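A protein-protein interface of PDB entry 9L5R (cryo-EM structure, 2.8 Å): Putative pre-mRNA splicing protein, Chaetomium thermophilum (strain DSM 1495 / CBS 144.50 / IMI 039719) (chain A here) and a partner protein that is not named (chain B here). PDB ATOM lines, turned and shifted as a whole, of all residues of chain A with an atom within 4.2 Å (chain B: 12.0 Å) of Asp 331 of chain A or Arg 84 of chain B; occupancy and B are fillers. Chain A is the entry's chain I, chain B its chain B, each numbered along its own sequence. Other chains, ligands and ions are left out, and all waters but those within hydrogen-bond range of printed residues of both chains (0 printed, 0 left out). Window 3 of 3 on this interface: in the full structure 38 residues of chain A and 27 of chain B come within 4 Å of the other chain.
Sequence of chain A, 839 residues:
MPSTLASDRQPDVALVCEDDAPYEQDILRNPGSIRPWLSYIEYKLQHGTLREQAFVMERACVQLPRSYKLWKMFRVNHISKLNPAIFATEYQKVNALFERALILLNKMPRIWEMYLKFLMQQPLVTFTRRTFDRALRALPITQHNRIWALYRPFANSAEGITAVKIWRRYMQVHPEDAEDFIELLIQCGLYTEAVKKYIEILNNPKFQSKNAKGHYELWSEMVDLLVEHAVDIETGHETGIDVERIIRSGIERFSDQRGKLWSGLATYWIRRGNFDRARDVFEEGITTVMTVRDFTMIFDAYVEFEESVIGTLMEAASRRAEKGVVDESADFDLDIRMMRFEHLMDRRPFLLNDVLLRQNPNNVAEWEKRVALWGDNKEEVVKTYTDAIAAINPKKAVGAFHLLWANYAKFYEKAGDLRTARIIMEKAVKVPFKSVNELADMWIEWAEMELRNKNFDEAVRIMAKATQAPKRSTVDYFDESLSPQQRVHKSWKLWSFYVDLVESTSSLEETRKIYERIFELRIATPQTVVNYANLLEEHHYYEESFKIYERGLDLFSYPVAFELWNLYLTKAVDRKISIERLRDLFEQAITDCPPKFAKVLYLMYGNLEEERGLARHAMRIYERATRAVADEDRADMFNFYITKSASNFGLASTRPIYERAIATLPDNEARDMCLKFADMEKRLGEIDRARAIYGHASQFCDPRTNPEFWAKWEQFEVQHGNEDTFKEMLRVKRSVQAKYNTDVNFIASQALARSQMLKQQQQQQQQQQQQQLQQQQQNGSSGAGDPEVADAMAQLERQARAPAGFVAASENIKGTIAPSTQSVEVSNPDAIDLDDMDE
NH2 of Arg 84 of chain B lies within salt-bridge range of OD1 of Asp 331 of chain A (2.5 Å).
The side-chain carboxylate of Glu 83 of chain B is in salt-bridge range of the guanidinium group of Arg 87 of chain B, 3.5 Å away.
CE of Met 314 of chain A touches O of Arg 84 of chain B, at 3.9 Å.
Arg 84 of chain B touches Leu 334 of chain A.
Arg 84 of chain B touches Met 338 of chain A.
Arg 87 of chain B touches Met 338 of chain A.
Asp 331 of chain A touches just one residue of chain B: Arg 84 (2.5 Å).
Arg 84 of chain B touches just these residues of chain A: Met 314, Asp 331, Leu 334 and Met 338.
No residue of chain B comes within 4 Å of Val 326 of chain A.
No residue of chain B comes within 4 Å of Asp 327 of chain A.
No residue of chain B comes within 4 Å of Ser 329 of chain A.
Ala 330 of chain A touches none of the printed residues of chain B.
No residue of chain B comes within 4 Å of Phe 332 of chain A.
No residue of chain B comes within 4 Å of Asp 333 of chain A.
Of the printed residues of chain A, Arg 87 of chain B touches Met 338.
Of the printed residues of chain B, Met 314 of chain A touches Arg 84 (3.9 Å).
Of the printed residues of chain B, Met 338 of chain A touches Arg 84 (3.6 Å) and Arg 87 (3.95 Å).
The nearest residue of chain A that does not touch Arg 84 of chain B is Asp 335 of chain A (4.1 Å).
Of the 22 printed residues of chain B, 2 touch a printed residue of chain A.
Printed residues of chain A that touch a printed residue of chain B: Met 314, Asp 331, Leu 334 and Met 338.
Hydrophobic or aromatic side chains of chain A that line the printed part of chain B: Met 314, Leu 334 and Met 338.
Among the printed residues, 5 pairs touch across the chains.
Among the printed residues, Asp or Glu carboxylates within 4 Å of a Lys or Arg side-chain nitrogen of the other chain: Asp 331 of chain A with Arg 84 of chain B.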
ATOM      1  N   MET A 314      29.043  11.654   0.279  1.00  0.00           N
ATOM      2  CA  MET A 314      28.050  11.403  -0.772  1.00  0.00           C
ATOM      3  C   MET A 314      28.653  10.615  -1.919  1.00  0.00           C
ATOM      4  O   MET A 314      28.022   9.674  -2.412  1.00  0.00           O
ATOM      5  CB  MET A 314      27.407  12.664  -1.369  1.00  0.00           C
ATOM      6  CG  MET A 314      26.971  13.788  -0.492  1.00  0.00           C
ATOM      7  SD  MET A 314      25.659  13.396   0.668  1.00  0.00           S
ATOM      8  CE  MET A 314      25.068  15.053   0.987  1.00  0.00           C
ATOM      9  N   VAL A 326      25.900  -1.143   1.839  1.00  0.00           N
ATOM     10  CA  VAL A 326      25.410  -0.219   2.856  1.00  0.00           C
ATOM     11  C   VAL A 326      25.395  -0.964   4.183  1.00  0.00           C
ATOM     12  O   VAL A 326      25.238  -2.189   4.224  1.00  0.00           O
ATOM     13  CB  VAL A 326      24.016   0.346   2.468  1.00  0.00           C
ATOM     14  CG1 VAL A 326      22.933  -0.729   2.531  1.00  0.00           C
ATOM     15  CG2 VAL A 326      23.649   1.562   3.315  1.00  0.00           C
ATOM     16  N   ASP A 327      25.603  -0.228   5.270  1.00  0.00           N
ATOM     17  CA  ASP A 327      25.623  -0.806   6.609  1.00  0.00           C
ATOM     18  C   ASP A 327      25.217   0.277   7.604  1.00  0.00           C
ATOM     19  O   ASP A 327      24.748   1.353   7.219  1.00  0.00           O
ATOM     20  CB  ASP A 327      27.002  -1.395   6.928  1.00  0.00           C
ATOM     21  CG  ASP A 327      28.131  -0.419   6.654  1.00  0.00           C
ATOM     22  OD1 ASP A 327      27.895   0.583   5.947  1.00  0.00           O
ATOM     23  OD2 ASP A 327      29.255  -0.656   7.145  1.00  0.00           O
ATOM     24  N   SER A 329      27.317   1.855   9.534  1.00  0.00           N
ATOM     25  CA  SER A 329      28.359   2.873   9.550  1.00  0.00           C
ATOM     26  C   SER A 329      28.219   3.902   8.436  1.00  0.00           C
ATOM     27  O   SER A 329      28.960   4.891   8.438  1.00  0.00           O
ATOM     28  CB  SER A 329      29.738   2.212   9.462  1.00  0.00           C
ATOM     29  OG  SER A 329      30.773   3.160   9.649  1.00  0.00           O
ATOM     30  N   ALA A 330      27.312   3.694   7.481  1.00  0.00           N
ATOM     31  CA  ALA A 330      27.118   4.636   6.386  1.00  0.00           C
ATOM     32  C   ALA A 330      25.746   5.298   6.419  1.00  0.00           C
ATOM     33  O   ALA A 330      25.656   6.524   6.513  1.00  0.00           O
ATOM     34  CB  ALA A 330      27.333   3.926   5.042  1.00  0.00           C
ATOM     35  N   ASP A 331      24.666   4.512   6.373  1.00  0.00           N
ATOM     36  CA  ASP A 331      23.331   5.091   6.255  1.00  0.00           C
ATOM     37  C   ASP A 331      22.872   5.707   7.570  1.00  0.00           C
ATOM     38  O   ASP A 331      22.438   6.867   7.609  1.00  0.00           O
ATOM     39  CB  ASP A 331      22.340   4.026   5.786  1.00  0.00           C
ATOM     40  CG  ASP A 331      20.960   4.590   5.518  1.00  0.00           C
ATOM     41  OD1 ASP A 331      20.785   5.274   4.489  1.00  0.00           O
ATOM     42  OD2 ASP A 331      20.050   4.347   6.338  1.00  0.00           O
ATOM     43  N   PHE A 332      22.963   4.942   8.661  1.00  0.00           N
ATOM     44  CA  PHE A 332      22.561   5.450   9.969  1.00  0.00           C
ATOM     45  C   PHE A 332      23.488   6.569  10.424  1.00  0.00           C
ATOM     46  O   PHE A 332      23.039   7.556  11.023  1.00  0.00           O
ATOM     47  CB  PHE A 332      22.549   4.304  10.981  1.00  0.00           C
ATOM     48  CG  PHE A 332      21.771   4.597  12.230  1.00  0.00           C
ATOM     49  CD1 PHE A 332      20.394   4.745  12.181  1.00  0.00           C
ATOM     50  CD2 PHE A 332      22.411   4.705  13.454  1.00  0.00           C
ATOM     51  CE1 PHE A 332      19.670   5.007  13.329  1.00  0.00           C
ATOM     52  CE2 PHE A 332      21.691   4.967  14.604  1.00  0.00           C
ATOM     53  CZ  PHE A 332      20.320   5.119  14.541  1.00  0.00           C
ATOM     54  N   ASP A 333      24.785   6.440  10.124  1.00  0.00           N
ATOM     55  CA  ASP A 333      25.739   7.494  10.447  1.00  0.00           C
ATOM     56  C   ASP A 333      25.439   8.773   9.674  1.00  0.00           C
ATOM     57  O   ASP A 333      25.487   9.866  10.242  1.00  0.00           O
ATOM     58  CB  ASP A 333      27.162   7.013  10.164  1.00  0.00           C
ATOM     59  CG  ASP A 333      28.194   7.701  11.034  1.00  0.00           C
ATOM     60  OD1 ASP A 333      27.802   8.525  11.886  1.00  0.00           O
ATOM     61  OD2 ASP A 333      29.398   7.412  10.869  1.00  0.00           O
ATOM     62  N   LEU A 334      25.103   8.659   8.388  1.00  0.00           N
ATOM     63  CA  LEU A 334      24.744   9.840   7.607  1.00  0.00           C
ATOM     64  C   LEU A 334      23.455  10.474   8.122  1.00  0.00           C
ATOM     65  O   LEU A 334      23.339  11.709   8.174  1.00  0.00           O
ATOM     66  CB  LEU A 334      24.624   9.455   6.132  1.00  0.00           C
ATOM     67  CG  LEU A 334      24.267  10.478   5.055  1.00  0.00           C
ATOM     68  CD1 LEU A 334      24.942  11.818   5.290  1.00  0.00           C
ATOM     69  CD2 LEU A 334      24.686   9.905   3.715  1.00  0.00           C
ATOM     70  N   ASP A 335      22.489   9.640   8.524  1.00  0.00           N
ATOM     71  CA  ASP A 335      21.241  10.147   9.087  1.00  0.00           C
ATOM     72  C   ASP A 335      21.491  10.936  10.367  1.00  0.00           C
ATOM     73  O   ASP A 335      20.946  12.031  10.548  1.00  0.00           O
ATOM     74  CB  ASP A 335      20.279   8.988   9.354  1.00  0.00           C
ATOM     75  CG  ASP A 335      19.549   8.538   8.106  1.00  0.00           C
ATOM     76  OD1 ASP A 335      18.984   9.402   7.402  1.00  0.00           O
ATOM     77  OD2 ASP A 335      19.539   7.321   7.826  1.00  0.00           O
ATOM     78  N   MET A 338      23.295  14.336   9.572  1.00  0.00           N
ATOM     79  CA  MET A 338      22.369  15.363   9.103  1.00  0.00           C
ATOM     80  C   MET A 338      21.382  15.783  10.182  1.00  0.00           C
ATOM     81  O   MET A 338      20.960  16.942  10.197  1.00  0.00           O
ATOM     82  CB  MET A 338      21.640  14.903   7.845  1.00  0.00           C
ATOM     83  CG  MET A 338      22.511  15.004   6.621  1.00  0.00           C
ATOM     84  SD  MET A 338      21.631  14.763   5.079  1.00  0.00           S
ATOM     85  CE  MET A 338      23.029  14.708   3.975  1.00  0.00           C
ATOM     86  N   SER B  72      15.251  -3.165  -4.292  1.00  0.00           N
ATOM     87  CA  SER B  72      14.472  -2.258  -3.455  1.00  0.00           C
ATOM     88  C   SER B  72      15.373  -1.439  -2.539  1.00  0.00           C
ATOM     89  O   SER B  72      15.136  -0.242  -2.333  1.00  0.00           O
ATOM     90  CB  SER B  72      13.450  -3.047  -2.636  1.00  0.00           C
ATOM     91  OG  SER B  72      14.091  -3.905  -1.709  1.00  0.00           O
ATOM     92  N   THR B  73      16.415  -2.067  -1.984  1.00  0.00           N
ATOM     93  CA  THR B  73      17.371  -1.341  -1.155  1.00  0.00           C
ATOM     94  C   THR B  73      18.143  -0.311  -1.972  1.00  0.00           C
ATOM     95  O   THR B  73      18.411   0.794  -1.488  1.00  0.00           O
ATOM     96  CB  THR B  73      18.334  -2.315  -0.477  1.00  0.00           C
ATOM     97  OG1 THR B  73      19.188  -2.910  -1.463  1.00  0.00           O
ATOM     98  CG2 THR B  73      17.564  -3.407   0.248  1.00  0.00           C
ATOM     99  N   LYS B  74      18.506  -0.656  -3.211  1.00  0.00           N
ATOM    100  CA  LYS B  74      19.188   0.295  -4.085  1.00  0.00           C
ATOM    101  C   LYS B  74      18.291   1.479  -4.433  1.00  0.00           C
ATOM    102  O   LYS B  74      18.751   2.626  -4.451  1.00  0.00           O
ATOM    103  CB  LYS B  74      19.659  -0.410  -5.358  1.00  0.00           C
ATOM    104  CG  LYS B  74      20.918  -1.240  -5.183  1.00  0.00           C
ATOM    105  CD  LYS B  74      21.377  -1.822  -6.510  1.00  0.00           C
ATOM    106  CE  LYS B  74      22.590  -2.719  -6.331  1.00  0.00           C
ATOM    107  NZ  LYS B  74      23.022  -3.331  -7.617  1.00  0.00           N
ATOM    108  N   ASN B  75      17.009   1.218  -4.708  1.00  0.00           N
ATOM    109  CA  ASN B  75      16.071   2.301  -4.997  1.00  0.00           C
ATOM    110  C   ASN B  75      15.851   3.189  -3.777  1.00  0.00           C
ATOM    111  O   ASN B  75      15.772   4.419  -3.902  1.00  0.00           O
ATOM    112  CB  ASN B  75      14.743   1.725  -5.489  1.00  0.00           C
ATOM    113  CG  ASN B  75      14.750   1.435  -6.975  1.00  0.00           C
ATOM    114  OD1 ASN B  75      15.421   2.116  -7.750  1.00  0.00           O
ATOM    115  ND2 ASN B  75      14.000   0.417  -7.383  1.00  0.00           N
ATOM    116  N   ALA B  76      15.749   2.581  -2.590  1.00  0.00           N
ATOM    117  CA  ALA B  76      15.607   3.358  -1.362  1.00  0.00           C
ATOM    118  C   ALA B  76      16.848   4.200  -1.094  1.00  0.00           C
ATOM    119  O   ALA B  76      16.740   5.354  -0.667  1.00  0.00           O
ATOM    120  CB  ALA B  76      15.323   2.428  -0.183  1.00  0.00           C
ATOM    121  N   ALA B  77      18.033   3.642  -1.353  1.00  0.00           N
ATOM    122  CA  ALA B  77      19.272   4.397  -1.197  1.00  0.00           C
ATOM    123  C   ALA B  77      19.353   5.547  -2.194  1.00  0.00           C
ATOM    124  O   ALA B  77      19.836   6.630  -1.856  1.00  0.00           O
ATOM    125  CB  ALA B  77      20.477   3.469  -1.349  1.00  0.00           C
ATOM    126  N   LEU B  78      18.884   5.328  -3.428  1.00  0.00           N
ATOM    127  CA  LEU B  78      18.887   6.395  -4.426  1.00  0.00           C
ATOM    128  C   LEU B  78      17.932   7.524  -4.046  1.00  0.00           C
ATOM    129  O   LEU B  78      18.277   8.705  -4.178  1.00  0.00           O
ATOM    130  CB  LEU B  78      18.526   5.828  -5.799  1.00  0.00           C
ATOM    131  CG  LEU B  78      19.659   5.137  -6.560  1.00  0.00           C
ATOM    132  CD1 LEU B  78      19.131   4.472  -7.822  1.00  0.00           C
ATOM    133  CD2 LEU B  78      20.764   6.127  -6.893  1.00  0.00           C
ATOM    134  N   THR B  79      16.731   7.180  -3.568  1.00  0.00           N
ATOM    135  CA  THR B  79      15.791   8.208  -3.120  1.00  0.00           C
ATOM    136  C   THR B  79      16.318   8.944  -1.892  1.00  0.00           C
ATOM    137  O   THR B  79      16.164  10.170  -1.779  1.00  0.00           O
ATOM    138  CB  THR B  79      14.426   7.586  -2.824  1.00  0.00           C
ATOM    139  OG1 THR B  79      14.584   6.486  -1.921  1.00  0.00           O
ATOM    140  CG2 THR B  79      13.773   7.096  -4.109  1.00  0.00           C
ATOM    141  N   ALA B  80      16.952   8.213  -0.970  1.00  0.00           N
ATOM    142  CA  ALA B  80      17.551   8.841   0.202  1.00  0.00           C
ATOM    143  C   ALA B  80      18.687   9.774  -0.193  1.00  0.00           C
ATOM    144  O   ALA B  80      18.828  10.856   0.379  1.00  0.00           O
ATOM    145  CB  ALA B  80      18.044   7.771   1.175  1.00  0.00           C
ATOM    146  N   ALA B  81      19.496   9.381  -1.181  1.00  0.00           N
ATOM    147  CA  ALA B  81      20.576  10.241  -1.653  1.00  0.00           C
ATOM    148  C   ALA B  81      20.046  11.474  -2.373  1.00  0.00           C
ATOM    149  O   ALA B  81      20.650  12.548  -2.278  1.00  0.00           O
ATOM    150  CB  ALA B  81      21.512   9.453  -2.570  1.00  0.00           C
ATOM    151  N   GLN B  82      18.933  11.341  -3.101  1.00  0.00           N
ATOM    152  CA  GLN B  82      18.296  12.511  -3.703  1.00  0.00           C
ATOM    153  C   GLN B  82      17.797  13.476  -2.634  1.00  0.00           C
ATOM    154  O   GLN B  82      17.985  14.698  -2.747  1.00  0.00           O
ATOM    155  CB  GLN B  82      17.146  12.072  -4.608  1.00  0.00           C
ATOM    156  CG  GLN B  82      17.587  11.517  -5.951  1.00  0.00           C
ATOM    157  CD  GLN B  82      16.417  11.096  -6.817  1.00  0.00           C
ATOM    158  OE1 GLN B  82      15.264  11.143  -6.389  1.00  0.00           O
ATOM    159  NE2 GLN B  82      16.708  10.680  -8.044  1.00  0.00           N
ATOM    160  N   GLU B  83      17.173  12.943  -1.579  1.00  0.00           N
ATOM    161  CA  GLU B  83      16.750  13.781  -0.458  1.00  0.00           C
ATOM    162  C   GLU B  83      17.949  14.414   0.243  1.00  0.00           C
ATOM    163  O   GLU B  83      17.881  15.563   0.690  1.00  0.00           O
ATOM    164  CB  GLU B  83      15.928  12.957   0.533  1.00  0.00           C
ATOM    165  CG  GLU B  83      14.501  12.691   0.090  1.00  0.00           C
ATOM    166  CD  GLU B  83      13.697  11.951   1.141  1.00  0.00           C
ATOM    167  OE1 GLU B  83      14.151  11.890   2.303  1.00  0.00           O
ATOM    168  OE2 GLU B  83      12.613  11.429   0.806  1.00  0.00           O
ATOM    169  N   ARG B  84      19.053  13.672   0.342  1.00  0.00           N
ATOM    170  CA  ARG B  84      20.268  14.188   0.963  1.00  0.00           C
ATOM    171  C   ARG B  84      20.865  15.327   0.148  1.00  0.00           C
ATOM    172  O   ARG B  84      21.345  16.316   0.711  1.00  0.00           O
ATOM    173  CB  ARG B  84      21.282  13.057   1.124  1.00  0.00           C
ATOM    174  CG  ARG B  84      21.039  12.169   2.332  1.00  0.00           C
ATOM    175  CD  ARG B  84      21.584  10.776   2.090  1.00  0.00           C
ATOM    176  NE  ARG B  84      21.110   9.818   3.081  1.00  0.00           N
ATOM    177  CZ  ARG B  84      21.088   8.504   2.901  1.00  0.00           C
ATOM    178  NH1 ARG B  84      21.505   7.955   1.771  1.00  0.00           N
ATOM    179  NH2 ARG B  84      20.638   7.722   3.877  1.00  0.00           N
ATOM    180  N   LEU B  85      20.853  15.201  -1.182  1.00  0.00           N
ATOM    181  CA  LEU B  85      21.340  16.278  -2.039  1.00  0.00           C
ATOM    182  C   LEU B  85      20.435  17.503  -1.960  1.00  0.00           C
ATOM    183  O   LEU B  85      20.918  18.643  -1.990  1.00  0.00           O
ATOM    184  CB  LEU B  85      21.457  15.788  -3.482  1.00  0.00           C
ATOM    185  CG  LEU B  85      22.719  14.993  -3.821  1.00  0.00           C
ATOM    186  CD1 LEU B  85      22.701  14.555  -5.277  1.00  0.00           C
ATOM    187  CD2 LEU B  85      23.965  15.810  -3.518  1.00  0.00           C
ATOM    188  N   ALA B  86      19.118  17.286  -1.862  1.00  0.00           N
ATOM    189  CA  ALA B  86      18.195  18.403  -1.668  1.00  0.00           C
ATOM    190  C   ALA B  86      18.452  19.110  -0.340  1.00  0.00           C
ATOM    191  O   ALA B  86      18.447  20.347  -0.274  1.00  0.00           O
ATOM    192  CB  ALA B  86      16.751  17.911  -1.745  1.00  0.00           C
ATOM    193  N   ARG B  87      18.689  18.337   0.725  1.00  0.00           N
ATOM    194  CA  ARG B  87      19.029  18.916   2.021  1.00  0.00           C
ATOM    195  C   ARG B  87      20.359  19.657   1.964  1.00  0.00           C
ATOM    196  O   ARG B  87      20.518  20.701   2.600  1.00  0.00           O
ATOM    197  CB  ARG B  87      19.078  17.828   3.093  1.00  0.00           C
ATOM    198  CG  ARG B  87      17.724  17.270   3.495  1.00  0.00           C
ATOM    199  CD  ARG B  87      17.857  16.351   4.699  1.00  0.00           C
ATOM    200  NE  ARG B  87      16.697  15.483   4.858  1.00  0.00           N
ATOM    201  CZ  ARG B  87      16.750  14.158   4.874  1.00  0.00           C
ATOM    202  NH1 ARG B  87      17.897  13.513   4.744  1.00  0.00           N
ATOM    203  NH2 ARG B  87      15.626  13.465   5.025  1.00  0.00           N
ATOM    204  N   PHE B  88      21.323  19.122   1.210  1.00  0.00           N
ATOM    205  CA  PHE B  88      22.616  19.779   1.042  1.00  0.00           C
ATOM    206  C   PHE B  88      22.469  21.125   0.343  1.00  0.00           C
ATOM    207  O   PHE B  88      23.070  22.120   0.764  1.00  0.00           O
ATOM    208  CB  PHE B  88      23.554  18.863   0.254  1.00  0.00           C
ATOM    209  CG  PHE B  88      24.989  19.303   0.265  1.00  0.00           C
ATOM    210  CD1 PHE B  88      25.805  19.014   1.344  1.00  0.00           C
ATOM    211  CD2 PHE B  88      25.525  19.988  -0.814  1.00  0.00           C
ATOM    212  CE1 PHE B  88      27.129  19.410   1.354  1.00  0.00           C
ATOM    213  CE2 PHE B  88      26.849  20.388  -0.809  1.00  0.00           C
ATOM    214  CZ  PHE B  88      27.651  20.099   0.277  1.00  0.00           C
ATOM    215  N   ARG B  89      21.663  21.176  -0.720  1.00  0.00           N
ATOM    216  CA  ARG B  89      21.447  22.433  -1.433  1.00  0.00           C
ATOM    217  C   ARG B  89      20.687  23.442  -0.574  1.00  0.00           C
ATOM    218  O   ARG B  89      21.013  24.638  -0.577  1.00  0.00           O
ATOM    219  CB  ARG B  89      20.708  22.169  -2.743  1.00  0.00           C
ATOM    220  CG  ARG B  89      21.577  21.529  -3.811  1.00  0.00           C
ATOM    221  CD  ARG B  89      20.743  20.973  -4.951  1.00  0.00           C
ATOM    222  NE  ARG B  89      21.564  20.259  -5.921  1.00  0.00           N
ATOM    223  CZ  ARG B  89      21.108  19.325  -6.744  1.00  0.00           C
ATOM    224  NH1 ARG B  89      19.835  18.963  -6.742  1.00  0.00           N
ATOM    225  NH2 ARG B  89      21.949  18.740  -7.591  1.00  0.00           N
ATOM    226  N   ALA B  90      19.679  22.977   0.171  1.00  0.00           N
ATOM    227  CA  ALA B  90      18.942  23.868   1.064  1.00  0.00           C
ATOM    228  C   ALA B  90      19.835  24.396   2.181  1.00  0.00           C
ATOM    229  O   ALA B  90      19.744  25.572   2.555  1.00  0.00           O
ATOM    230  CB  ALA B  90      17.728  23.142   1.645  1.00  0.00           C
ATOM    231  N   LEU B  91      20.710  23.541   2.717  1.00  0.00           N
ATOM    232  CA  LEU B  91      21.638  23.959   3.760  1.00  0.00           C
ATOM    233  C   LEU B  91      22.656  24.953   3.214  1.00  0.00           C
ATOM    234  O   LEU B  91      23.025  25.907   3.906  1.00  0.00           O
ATOM    235  CB  LEU B  91      22.320  22.723   4.359  1.00  0.00           C
ATOM    236  CG  LEU B  91      23.152  22.777   5.646  1.00  0.00           C
ATOM    237  CD1 LEU B  91      23.059  21.436   6.360  1.00  0.00           C
ATOM    238  CD2 LEU B  91      24.611  23.120   5.396  1.00  0.00           C
ATOM    239  N   GLN B  92      23.102  24.754   1.968  1.00  0.00           N
ATOM    240  CA  GLN B  92      23.992  25.713   1.319  1.00  0.00           C
ATOM    241  C   GLN B  92      23.325  27.075   1.168  1.00  0.00           C
ATOM    242  O   GLN B  92      23.927  28.112   1.476  1.00  0.00           O
ATOM    243  CB  GLN B  92      24.424  25.184  -0.050  1.00  0.00           C
ATOM    244  CG  GLN B  92      25.661  24.308  -0.040  1.00  0.00           C
ATOM    245  CD  GLN B  92      26.094  23.900  -1.434  1.00  0.00           C
ATOM    246  OE1 GLN B  92      25.301  23.931  -2.375  1.00  0.00           O
ATOM    247  NE2 GLN B  92      27.361  23.527  -1.576  1.00  0.00           N
ATOM    248  N   ALA B  93      22.074  27.087   0.693  1.00  0.00           N
ATOM    249  CA  ALA B  93      21.361  28.350   0.501  1.00  0.00           C
ATOM    250  C   ALA B  93      21.108  29.060   1.826  1.00  0.00           C
ATOM    251  O   ALA B  93      21.295  30.281   1.931  1.00  0.00           O
ATOM    252  CB  ALA B  93      20.045  28.100  -0.236  1.00  0.00           C
